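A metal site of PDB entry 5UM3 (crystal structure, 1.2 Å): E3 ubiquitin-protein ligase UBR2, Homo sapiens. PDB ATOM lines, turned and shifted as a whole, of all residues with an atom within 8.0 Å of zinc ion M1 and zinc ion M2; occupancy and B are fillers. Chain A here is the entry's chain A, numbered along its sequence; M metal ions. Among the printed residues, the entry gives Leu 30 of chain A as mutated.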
ATOM      1  N   SER A   5     -19.666  16.418 -20.801  1.00  0.00           N
ATOM      2  CA  SER A   5     -19.508  17.777 -21.294  1.00  0.00           C
ATOM      3  C   SER A   5     -18.644  17.793 -22.542  1.00  0.00           C
ATOM      4  O   SER A   5     -17.898  16.855 -22.828  1.00  0.00           O
ATOM      5  CB  SER A   5     -18.914  18.707 -20.216  1.00  0.00           C
ATOM      6  OG  SER A   5     -17.627  18.282 -19.800  1.00  0.00           O
ATOM      7  N   LEU A   6     -18.772  18.877 -23.297  1.00  0.00           N
ATOM      8  CA  LEU A   6     -17.935  19.106 -24.484  1.00  0.00           C
ATOM      9  C   LEU A   6     -16.590  19.688 -24.057  1.00  0.00           C
ATOM     10  O   LEU A   6     -16.536  20.610 -23.251  1.00  0.00           O
ATOM     11  CB  LEU A   6     -18.623  20.107 -25.402  1.00  0.00           C
ATOM     12  CG  LEU A   6     -19.847  19.639 -26.176  1.00  0.00           C
ATOM     13  CD1 LEU A   6     -20.565  20.823 -26.800  1.00  0.00           C
ATOM     14  CD2 LEU A   6     -19.453  18.650 -27.263  1.00  0.00           C
ATOM     15  N   CYS A   7     -15.517  19.158 -24.627  1.00  0.00           N
ATOM     16  CA  CYS A   7     -14.202  19.773 -24.417  1.00  0.00           C
ATOM     17  C   CYS A   7     -14.161  21.171 -25.031  1.00  0.00           C
ATOM     18  O   CYS A   7     -13.910  22.161 -24.336  1.00  0.00           O
ATOM     19  CB  CYS A   7     -13.118  18.912 -25.039  1.00  0.00           C
ATOM     20  SG  CYS A   7     -11.484  19.699 -24.957  1.00  0.00           S
ATOM     21  N   GLY A   8     -14.433  21.270 -26.322  1.00  0.00           N
ATOM     22  CA  GLY A   8     -14.478  22.528 -27.022  1.00  0.00           C
ATOM     23  C   GLY A   8     -13.159  23.252 -27.165  1.00  0.00           C
ATOM     24  O   GLY A   8     -13.169  24.409 -27.585  1.00  0.00           O
ATOM     25  N   ARG A   9     -12.028  22.631 -26.858  1.00  0.00           N
ATOM     26  CA  ARG A   9     -10.740  23.333 -26.919  1.00  0.00           C
ATOM     27  C   ARG A   9     -10.484  23.816 -28.340  1.00  0.00           C
ATOM     28  O   ARG A   9     -10.551  23.041 -29.295  1.00  0.00           O
ATOM     29  CB  ARG A   9      -9.603  22.428 -26.458  1.00  0.00           C
ATOM     30  CG  ARG A   9      -8.245  23.138 -26.447  1.00  0.00           C
ATOM     31  CD  ARG A   9      -7.189  22.352 -25.693  1.00  0.00           C
ATOM     32  NE  ARG A   9      -5.954  23.117 -25.524  1.00  0.00           N
ATOM     33  CZ  ARG A   9      -5.116  22.999 -24.503  1.00  0.00           C
ATOM     34  NH1 ARG A   9      -5.353  22.143 -23.513  1.00  0.00           N
ATOM     35  NH2 ARG A   9      -4.025  23.756 -24.449  1.00  0.00           N
ATOM     36  N   VAL A  10     -10.171  25.098 -28.475  1.00  0.00           N
ATOM     37  CA  VAL A  10      -9.888  25.700 -29.771  1.00  0.00           C
ATOM     38  C   VAL A  10      -8.421  25.469 -30.094  1.00  0.00           C
ATOM     39  O   VAL A  10      -7.547  25.846 -29.315  1.00  0.00           O
ATOM     40  CB  VAL A  10     -10.221  27.198 -29.751  1.00  0.00           C
ATOM     41  CG1 VAL A  10      -9.807  27.827 -31.055  1.00  0.00           C
ATOM     42  CG2 VAL A  10     -11.703  27.406 -29.516  1.00  0.00           C
ATOM     43  N   PHE A  11      -8.163  24.835 -31.240  1.00  0.00           N
ATOM     44  CA  PHE A  11      -6.788  24.523 -31.603  1.00  0.00           C
ATOM     45  C   PHE A  11      -6.023  25.770 -31.988  1.00  0.00           C
ATOM     46  O   PHE A  11      -6.530  26.639 -32.690  1.00  0.00           O
ATOM     47  CB  PHE A  11      -6.752  23.531 -32.760  1.00  0.00           C
ATOM     48  CG  PHE A  11      -7.288  22.182 -32.414  1.00  0.00           C
ATOM     49  CD1 PHE A  11      -6.707  21.443 -31.390  1.00  0.00           C
ATOM     50  CD2 PHE A  11      -8.363  21.636 -33.099  1.00  0.00           C
ATOM     51  CE1 PHE A  11      -7.204  20.200 -31.071  1.00  0.00           C
ATOM     52  CE2 PHE A  11      -8.834  20.382 -32.773  1.00  0.00           C
ATOM     53  CZ  PHE A  11      -8.266  19.676 -31.771  1.00  0.00           C
ATOM     54  N   LEU A  30     -11.966  15.570 -34.647  1.00  0.00           N
ATOM     55  CA  LEU A  30     -10.619  15.687 -34.081  1.00  0.00           C
ATOM     56  C   LEU A  30     -10.692  15.719 -32.567  1.00  0.00           C
ATOM     57  O   LEU A  30     -11.684  16.147 -31.980  1.00  0.00           O
ATOM     58  CB  LEU A  30      -9.932  16.958 -34.577  1.00  0.00           C
ATOM     59  CG  LEU A  30      -9.686  16.989 -36.089  1.00  0.00           C
ATOM     60  CD1 LEU A  30      -9.241  18.391 -36.514  1.00  0.00           C
ATOM     61  CD2 LEU A  30      -8.670  15.921 -36.523  1.00  0.00           C
ATOM     62  N   LEU A  31      -9.594  15.276 -31.938  1.00  0.00           N
ATOM     63  CA  LEU A  31      -9.401  15.360 -30.497  1.00  0.00           C
ATOM     64  C   LEU A  31      -8.120  16.112 -30.167  1.00  0.00           C
ATOM     65  O   LEU A  31      -7.125  16.007 -30.884  1.00  0.00           O
ATOM     66  CB  LEU A  31      -9.287  13.971 -29.897  1.00  0.00           C
ATOM     67  CG  LEU A  31     -10.523  13.099 -30.070  1.00  0.00           C
ATOM     68  CD1 LEU A  31     -10.234  11.660 -29.697  1.00  0.00           C
ATOM     69  CD2 LEU A  31     -11.678  13.631 -29.223  1.00  0.00           C
ATOM     70  N   CYS A  32      -8.167  16.870 -29.075  1.00  0.00           N
ATOM     71  CA  CYS A  32      -6.942  17.433 -28.518  1.00  0.00           C
ATOM     72  C   CYS A  32      -6.111  16.340 -27.859  1.00  0.00           C
ATOM     73  O   CYS A  32      -6.585  15.227 -27.584  1.00  0.00           O
ATOM     74  CB  CYS A  32      -7.253  18.552 -27.524  1.00  0.00           C
ATOM     75  SG  CYS A  32      -7.980  18.024 -25.952  1.00  0.00           S
ATOM     76  N   MET A  33      -4.851  16.663 -27.576  1.00  0.00           N
ATOM     77  CA  MET A  33      -3.939  15.647 -27.052  1.00  0.00           C
ATOM     78  C   MET A  33      -4.432  15.093 -25.722  1.00  0.00           C
ATOM     79  O   MET A  33      -4.401  13.870 -25.504  1.00  0.00           O
ATOM     80  CB  MET A  33      -2.540  16.250 -26.910  1.00  0.00           C
ATOM     81  CG  MET A  33      -1.416  15.223 -26.784  1.00  0.00           C
ATOM     82  SD  MET A  33       0.230  15.933 -26.829  1.00  0.00           S
ATOM     83  CE  MET A  33       0.178  16.521 -25.174  1.00  0.00           C
ATOM     84  N   GLU A  34      -4.889  15.968 -24.823  1.00  0.00           N
ATOM     85  CA  GLU A  34      -5.372  15.537 -23.498  1.00  0.00           C
ATOM     86  C   GLU A  34      -6.538  14.570 -23.634  1.00  0.00           C
ATOM     87  O   GLU A  34      -6.606  13.538 -22.949  1.00  0.00           O
ATOM     88  CB  GLU A  34      -5.782  16.781 -22.682  1.00  0.00           C
ATOM     89  CG  GLU A  34      -6.422  16.486 -21.305  1.00  0.00           C
ATOM     90  CD  GLU A  34      -6.943  17.723 -20.554  1.00  0.00           C
ATOM     91  OE1 GLU A  34      -7.489  18.669 -21.171  1.00  0.00           O
ATOM     92  OE2 GLU A  34      -6.835  17.718 -19.301  1.00  0.00           O
ATOM     93  N   CYS A  35      -7.510  14.906 -24.479  1.00  0.00           N
ATOM     94  CA  CYS A  35      -8.674  14.051 -24.663  1.00  0.00           C
ATOM     95  C   CYS A  35      -8.288  12.740 -25.342  1.00  0.00           C
ATOM     96  O   CYS A  35      -8.712  11.658 -24.916  1.00  0.00           O
ATOM     97  CB  CYS A  35      -9.728  14.793 -25.465  1.00  0.00           C
ATOM     98  SG  CYS A  35     -10.449  16.148 -24.463  1.00  0.00           S
ATOM     99  N   PHE A  36      -7.494  12.827 -26.400  1.00  0.00           N
ATOM    100  CA  PHE A  36      -7.077  11.633 -27.114  1.00  0.00           C
ATOM    101  C   PHE A  36      -6.438  10.627 -26.167  1.00  0.00           C
ATOM    102  O   PHE A  36      -6.813   9.442 -26.157  1.00  0.00           O
ATOM    103  CB  PHE A  36      -6.105  12.025 -28.220  1.00  0.00           C
ATOM    104  CG  PHE A  36      -5.504  10.861 -28.934  1.00  0.00           C
ATOM    105  CD1 PHE A  36      -6.256  10.082 -29.817  1.00  0.00           C
ATOM    106  CD2 PHE A  36      -4.175  10.510 -28.711  1.00  0.00           C
ATOM    107  CE1 PHE A  36      -5.697   9.001 -30.460  1.00  0.00           C
ATOM    108  CE2 PHE A  36      -3.603   9.416 -29.362  1.00  0.00           C
ATOM    109  CZ  PHE A  36      -4.377   8.670 -30.234  1.00  0.00           C
ATOM    110  N   GLY A  38      -6.712  10.283 -23.022  1.00  0.00           N
ATOM    111  CA  GLY A  38      -7.634   9.822 -21.997  1.00  0.00           C
ATOM    112  C   GLY A  38      -8.849   9.117 -22.561  1.00  0.00           C
ATOM    113  O   GLY A  38      -9.825   8.903 -21.853  1.00  0.00           O
ATOM    114  N   SER A  39      -8.775   8.691 -23.830  1.00  0.00           N
ATOM    115  CA  SER A  39      -9.898   8.099 -24.545  1.00  0.00           C
ATOM    116  C   SER A  39      -9.526   6.698 -25.011  1.00  0.00           C
ATOM    117  O   SER A  39      -8.366   6.294 -24.993  1.00  0.00           O
ATOM    118  CB  SER A  39     -10.284   8.944 -25.764  1.00  0.00           C
ATOM    119  OG  SER A  39      -9.381   8.704 -26.825  1.00  0.00           O
ATOM    120  N   PHE A  56     -11.927  22.920 -33.373  1.00  0.00           N
ATOM    121  CA  PHE A  56     -11.919  22.594 -31.951  1.00  0.00           C
ATOM    122  C   PHE A  56     -11.965  21.092 -31.760  1.00  0.00           C
ATOM    123  O   PHE A  56     -12.296  20.314 -32.665  1.00  0.00           O
ATOM    124  CB  PHE A  56     -13.054  23.289 -31.203  1.00  0.00           C
ATOM    125  CG  PHE A  56     -14.233  23.548 -32.059  1.00  0.00           C
ATOM    126  CD1 PHE A  56     -14.477  24.807 -32.567  1.00  0.00           C
ATOM    127  CD2 PHE A  56     -15.096  22.517 -32.395  1.00  0.00           C
ATOM    128  CE1 PHE A  56     -15.560  25.041 -33.379  1.00  0.00           C
ATOM    129  CE2 PHE A  56     -16.170  22.731 -33.211  1.00  0.00           C
ATOM    130  CZ  PHE A  56     -16.410  24.005 -33.712  1.00  0.00           C
ATOM    131  N   CYS A  57     -11.596  20.703 -30.547  1.00  0.00           N
ATOM    132  CA  CYS A  57     -11.705  19.334 -30.107  1.00  0.00           C
ATOM    133  C   CYS A  57     -13.169  18.925 -30.073  1.00  0.00           C
ATOM    134  O   CYS A  57     -14.000  19.668 -29.574  1.00  0.00           O
ATOM    135  CB  CYS A  57     -11.096  19.209 -28.710  1.00  0.00           C
ATOM    136  SG  CYS A  57     -11.226  17.534 -28.049  1.00  0.00           S
ATOM    137  N   ASP A  58     -13.448  17.746 -30.617  1.00  0.00           N
ATOM    138  CA  ASP A  58     -14.796  17.198 -30.693  1.00  0.00           C
ATOM    139  C   ASP A  58     -15.086  16.183 -29.589  1.00  0.00           C
ATOM    140  O   ASP A  58     -16.062  15.433 -29.714  1.00  0.00           O
ATOM    141  CB  ASP A  58     -14.999  16.536 -32.055  1.00  0.00           C
ATOM    142  CG  ASP A  58     -15.033  17.541 -33.190  1.00  0.00           C
ATOM    143  OD1 ASP A  58     -15.779  18.533 -33.085  1.00  0.00           O
ATOM    144  OD2 ASP A  58     -14.327  17.324 -34.184  1.00  0.00           O
ATOM    145  N   CYS A  59     -14.275  16.134 -28.546  1.00  0.00           N
ATOM    146  CA  CYS A  59     -14.569  15.262 -27.428  1.00  0.00           C
ATOM    147  C   CYS A  59     -15.894  15.677 -26.785  1.00  0.00           C
ATOM    148  O   CYS A  59     -16.133  16.859 -26.520  1.00  0.00           O
ATOM    149  CB  CYS A  59     -13.451  15.312 -26.395  1.00  0.00           C
ATOM    150  SG  CYS A  59     -13.637  14.116 -25.094  1.00  0.00           S
ATOM    151  N   GLY A  60     -16.742  14.696 -26.550  1.00  0.00           N
ATOM    152  CA  GLY A  60     -18.042  14.938 -25.987  1.00  0.00           C
ATOM    153  C   GLY A  60     -19.138  15.129 -27.018  1.00  0.00           C
ATOM    154  O   GLY A  60     -20.306  15.289 -26.628  1.00  0.00           O
ATOM    155  N   PRO A  69     -17.170   8.472 -27.491  1.00  0.00           N
ATOM    156  CA  PRO A  69     -17.232   9.918 -27.738  1.00  0.00           C
ATOM    157  C   PRO A  69     -16.648  10.776 -26.638  1.00  0.00           C
ATOM    158  O   PRO A  69     -16.293  11.928 -26.914  1.00  0.00           O
ATOM    159  CB  PRO A  69     -18.731  10.187 -27.909  1.00  0.00           C
ATOM    160  CG  PRO A  69     -19.393   9.092 -27.164  1.00  0.00           C
ATOM    161  CD  PRO A  69     -18.517   7.886 -27.363  1.00  0.00           C
ATOM    162  N   TYR A  70     -16.518  10.264 -25.414  1.00  0.00           N
ATOM    163  CA  TYR A  70     -15.953  11.019 -24.304  1.00  0.00           C
ATOM    164  C   TYR A  70     -14.633  10.409 -23.841  1.00  0.00           C
ATOM    165  O   TYR A  70     -14.425   9.197 -23.917  1.00  0.00           O
ATOM    166  CB  TYR A  70     -16.879  11.007 -23.084  1.00  0.00           C
ATOM    167  CG  TYR A  70     -18.174  11.746 -23.250  1.00  0.00           C
ATOM    168  CD1 TYR A  70     -19.332  11.095 -23.663  1.00  0.00           C
ATOM    169  CD2 TYR A  70     -18.249  13.100 -22.945  1.00  0.00           C
ATOM    170  CE1 TYR A  70     -20.526  11.781 -23.784  1.00  0.00           C
ATOM    171  CE2 TYR A  70     -19.448  13.786 -23.049  1.00  0.00           C
ATOM    172  CZ  TYR A  70     -20.575  13.124 -23.472  1.00  0.00           C
ATOM    173  OH  TYR A  70     -21.747  13.822 -23.575  1.00  0.00           O
ATOM    174  N   CYS A  71     -13.792  11.255 -23.281  1.00  0.00           N
ATOM    175  CA  CYS A  71     -12.581  10.841 -22.593  1.00  0.00           C
ATOM    176  C   CYS A  71     -12.859  10.825 -21.084  1.00  0.00           C
ATOM    177  O   CYS A  71     -13.935  11.226 -20.632  1.00  0.00           O
ATOM    178  CB  CYS A  71     -11.418  11.780 -22.924  1.00  0.00           C
ATOM    179  SG  CYS A  71     -11.511  13.365 -22.042  1.00  0.00           S
ATOM    180  N   GLN A  72     -11.859  10.419 -20.302  1.00  0.00           N
ATOM    181  CA  GLN A  72     -12.031  10.331 -18.854  1.00  0.00           C
ATOM    182  C   GLN A  72     -12.323  11.690 -18.223  1.00  0.00           C
ATOM    183  O   GLN A  72     -12.997  11.757 -17.189  1.00  0.00           O
ATOM    184  CB  GLN A  72     -10.796   9.689 -18.209  1.00  0.00           C
ATOM    185  CG  GLN A  72      -9.442  10.399 -18.444  1.00  0.00           C
ATOM    186  CD  GLN A  72      -9.245  11.648 -17.582  1.00  0.00           C
ATOM    187  OE1 GLN A  72      -9.683  11.737 -16.433  1.00  0.00           O
ATOM    188  NE2 GLN A  72      -8.553  12.629 -18.133  1.00  0.00           N
ATOM    189  N   LYS A  73     -11.835  12.788 -18.811  1.00  0.00           N
ATOM    190  CA  LYS A  73     -12.071  14.104 -18.218  1.00  0.00           C
ATOM    191  C   LYS A  73     -13.501  14.575 -18.445  1.00  0.00           C
ATOM    192  O   LYS A  73     -14.104  15.203 -17.563  1.00  0.00           O
ATOM    193  CB  LYS A  73     -11.096  15.128 -18.803  1.00  0.00           C
ATOM    194  CG  LYS A  73     -11.243  16.516 -18.206  1.00  0.00           C
ATOM    195  CD  LYS A  73     -10.295  17.498 -18.838  1.00  0.00           C
ATOM    196  CE  LYS A  73     -10.358  18.827 -18.117  1.00  0.00           C
ATOM    197  NZ  LYS A  73      -9.514  19.870 -18.766  1.00  0.00           N
ATOM    198  N   HIS A  74     -14.055  14.283 -19.625  1.00  0.00           N
ATOM    199  CA  HIS A  74     -15.301  14.902 -20.033  1.00  0.00           C
ATOM    200  C   HIS A  74     -16.531  14.019 -19.894  1.00  0.00           C
ATOM    201  O   HIS A  74     -17.646  14.539 -19.998  1.00  0.00           O
ATOM    202  CB  HIS A  74     -15.159  15.438 -21.449  1.00  0.00           C
ATOM    203  CG  HIS A  74     -14.182  16.564 -21.514  1.00  0.00           C
ATOM    204  ND1 HIS A  74     -12.982  16.486 -22.196  1.00  0.00           N
ATOM    205  CD2 HIS A  74     -14.196  17.772 -20.916  1.00  0.00           C
ATOM    206  CE1 HIS A  74     -12.316  17.606 -22.015  1.00  0.00           C
ATOM    207  NE2 HIS A  74     -13.035  18.417 -21.254  1.00  0.00           N
ATOM    208  N   GLU A  75     -16.357  12.728 -19.637  1.00  0.00           N
ATOM    209  CA  GLU A  75     -17.523  11.856 -19.488  1.00  0.00           C
ATOM    210  C   GLU A  75     -18.302  12.206 -18.235  1.00  0.00           C
ATOM    211  O   GLU A  75     -19.467  11.846 -18.171  1.00  0.00           O
ATOM    212  CB  GLU A  75     -17.123  10.381 -19.437  1.00  0.00           C
ATOM    213  CG  GLU A  75     -16.307   9.984 -18.214  1.00  0.00           C
ATOM    214  CD  GLU A  75     -15.870   8.540 -18.227  1.00  0.00           C
ATOM    215  OE1 GLU A  75     -16.497   7.713 -18.915  1.00  0.00           O
ATOM    216  OE2 GLU A  75     -14.871   8.242 -17.542  1.00  0.00           O
ATOM    217  OXT GLU A  75     -17.791  12.820 -17.305  1.00  0.00           O
HETATM  218 ZN    ZN M   1     -10.310  18.000 -25.954  1.00  0.00          ZN
HETATM  219 ZN    ZN M   2     -12.275  15.019 -23.480  1.00  0.00          ZN
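O of His 74 sits at hydrogen-bond distance from N of Ser 5 (2.9 Å). The backbone NH (N) of Cys 7 lies within hydrogen-bond range of the backbone carbonyl oxygen (O) of Cys 59. The side-chain sulfur of Cys 7 sits close to the backbone NH of Arg 9 (3.5 Å). N of Cys 59 sits close to SG of Cys 57, at 3.4 Å. N of Lys 73 lies close to SG of Cys 71 (3.3 Å). The backbone NH of Cys 57 is in hydrogen-bond range of the backbone carbonyl oxygen of Arg 9, at 2.9 Å.
Of the 28 residues printed, 4 come within 4 Å of zinc ion M1. The nearest printed residue that does not touch zinc ion M1 is Cys 59 (4.2 Å).
Four residues have an atom within 4 Å of zinc ion M2: Cys 35, Cys 59, Cys 71 and His 74. Along chain A the residues within 4 Å of zinc ion M2 span positions 35 to 74. The nearest printed residue that does not touch zinc ion M2 is Cys 7 (4.3 Å).
SG of Cys 7 is bound to zinc ion M1, 2.3 Å away. SG of Cys 32 binds zinc ion M1 (2.3 Å). The side-chain sulfur (SG) of Cys 57 is bound to zinc ion M1, 2.3 Å away. Zinc ion M1 is bound by the side-chain sulfur (SG) of Cys 35.
ND1 of His 74 binds zinc ion M2 (2.1 Å). The side-chain sulfur (SG) of Cys 59 binds zinc ion M2, 2.3 Å away. SG of Cys 71 is bound to zinc ion M2, at 2.3 Å. The side-chain sulfur (SG) of Cys 35 is bound to zinc ion M2, at 2.4 Å. Zinc ion M2 has four donor atoms within binding distance.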
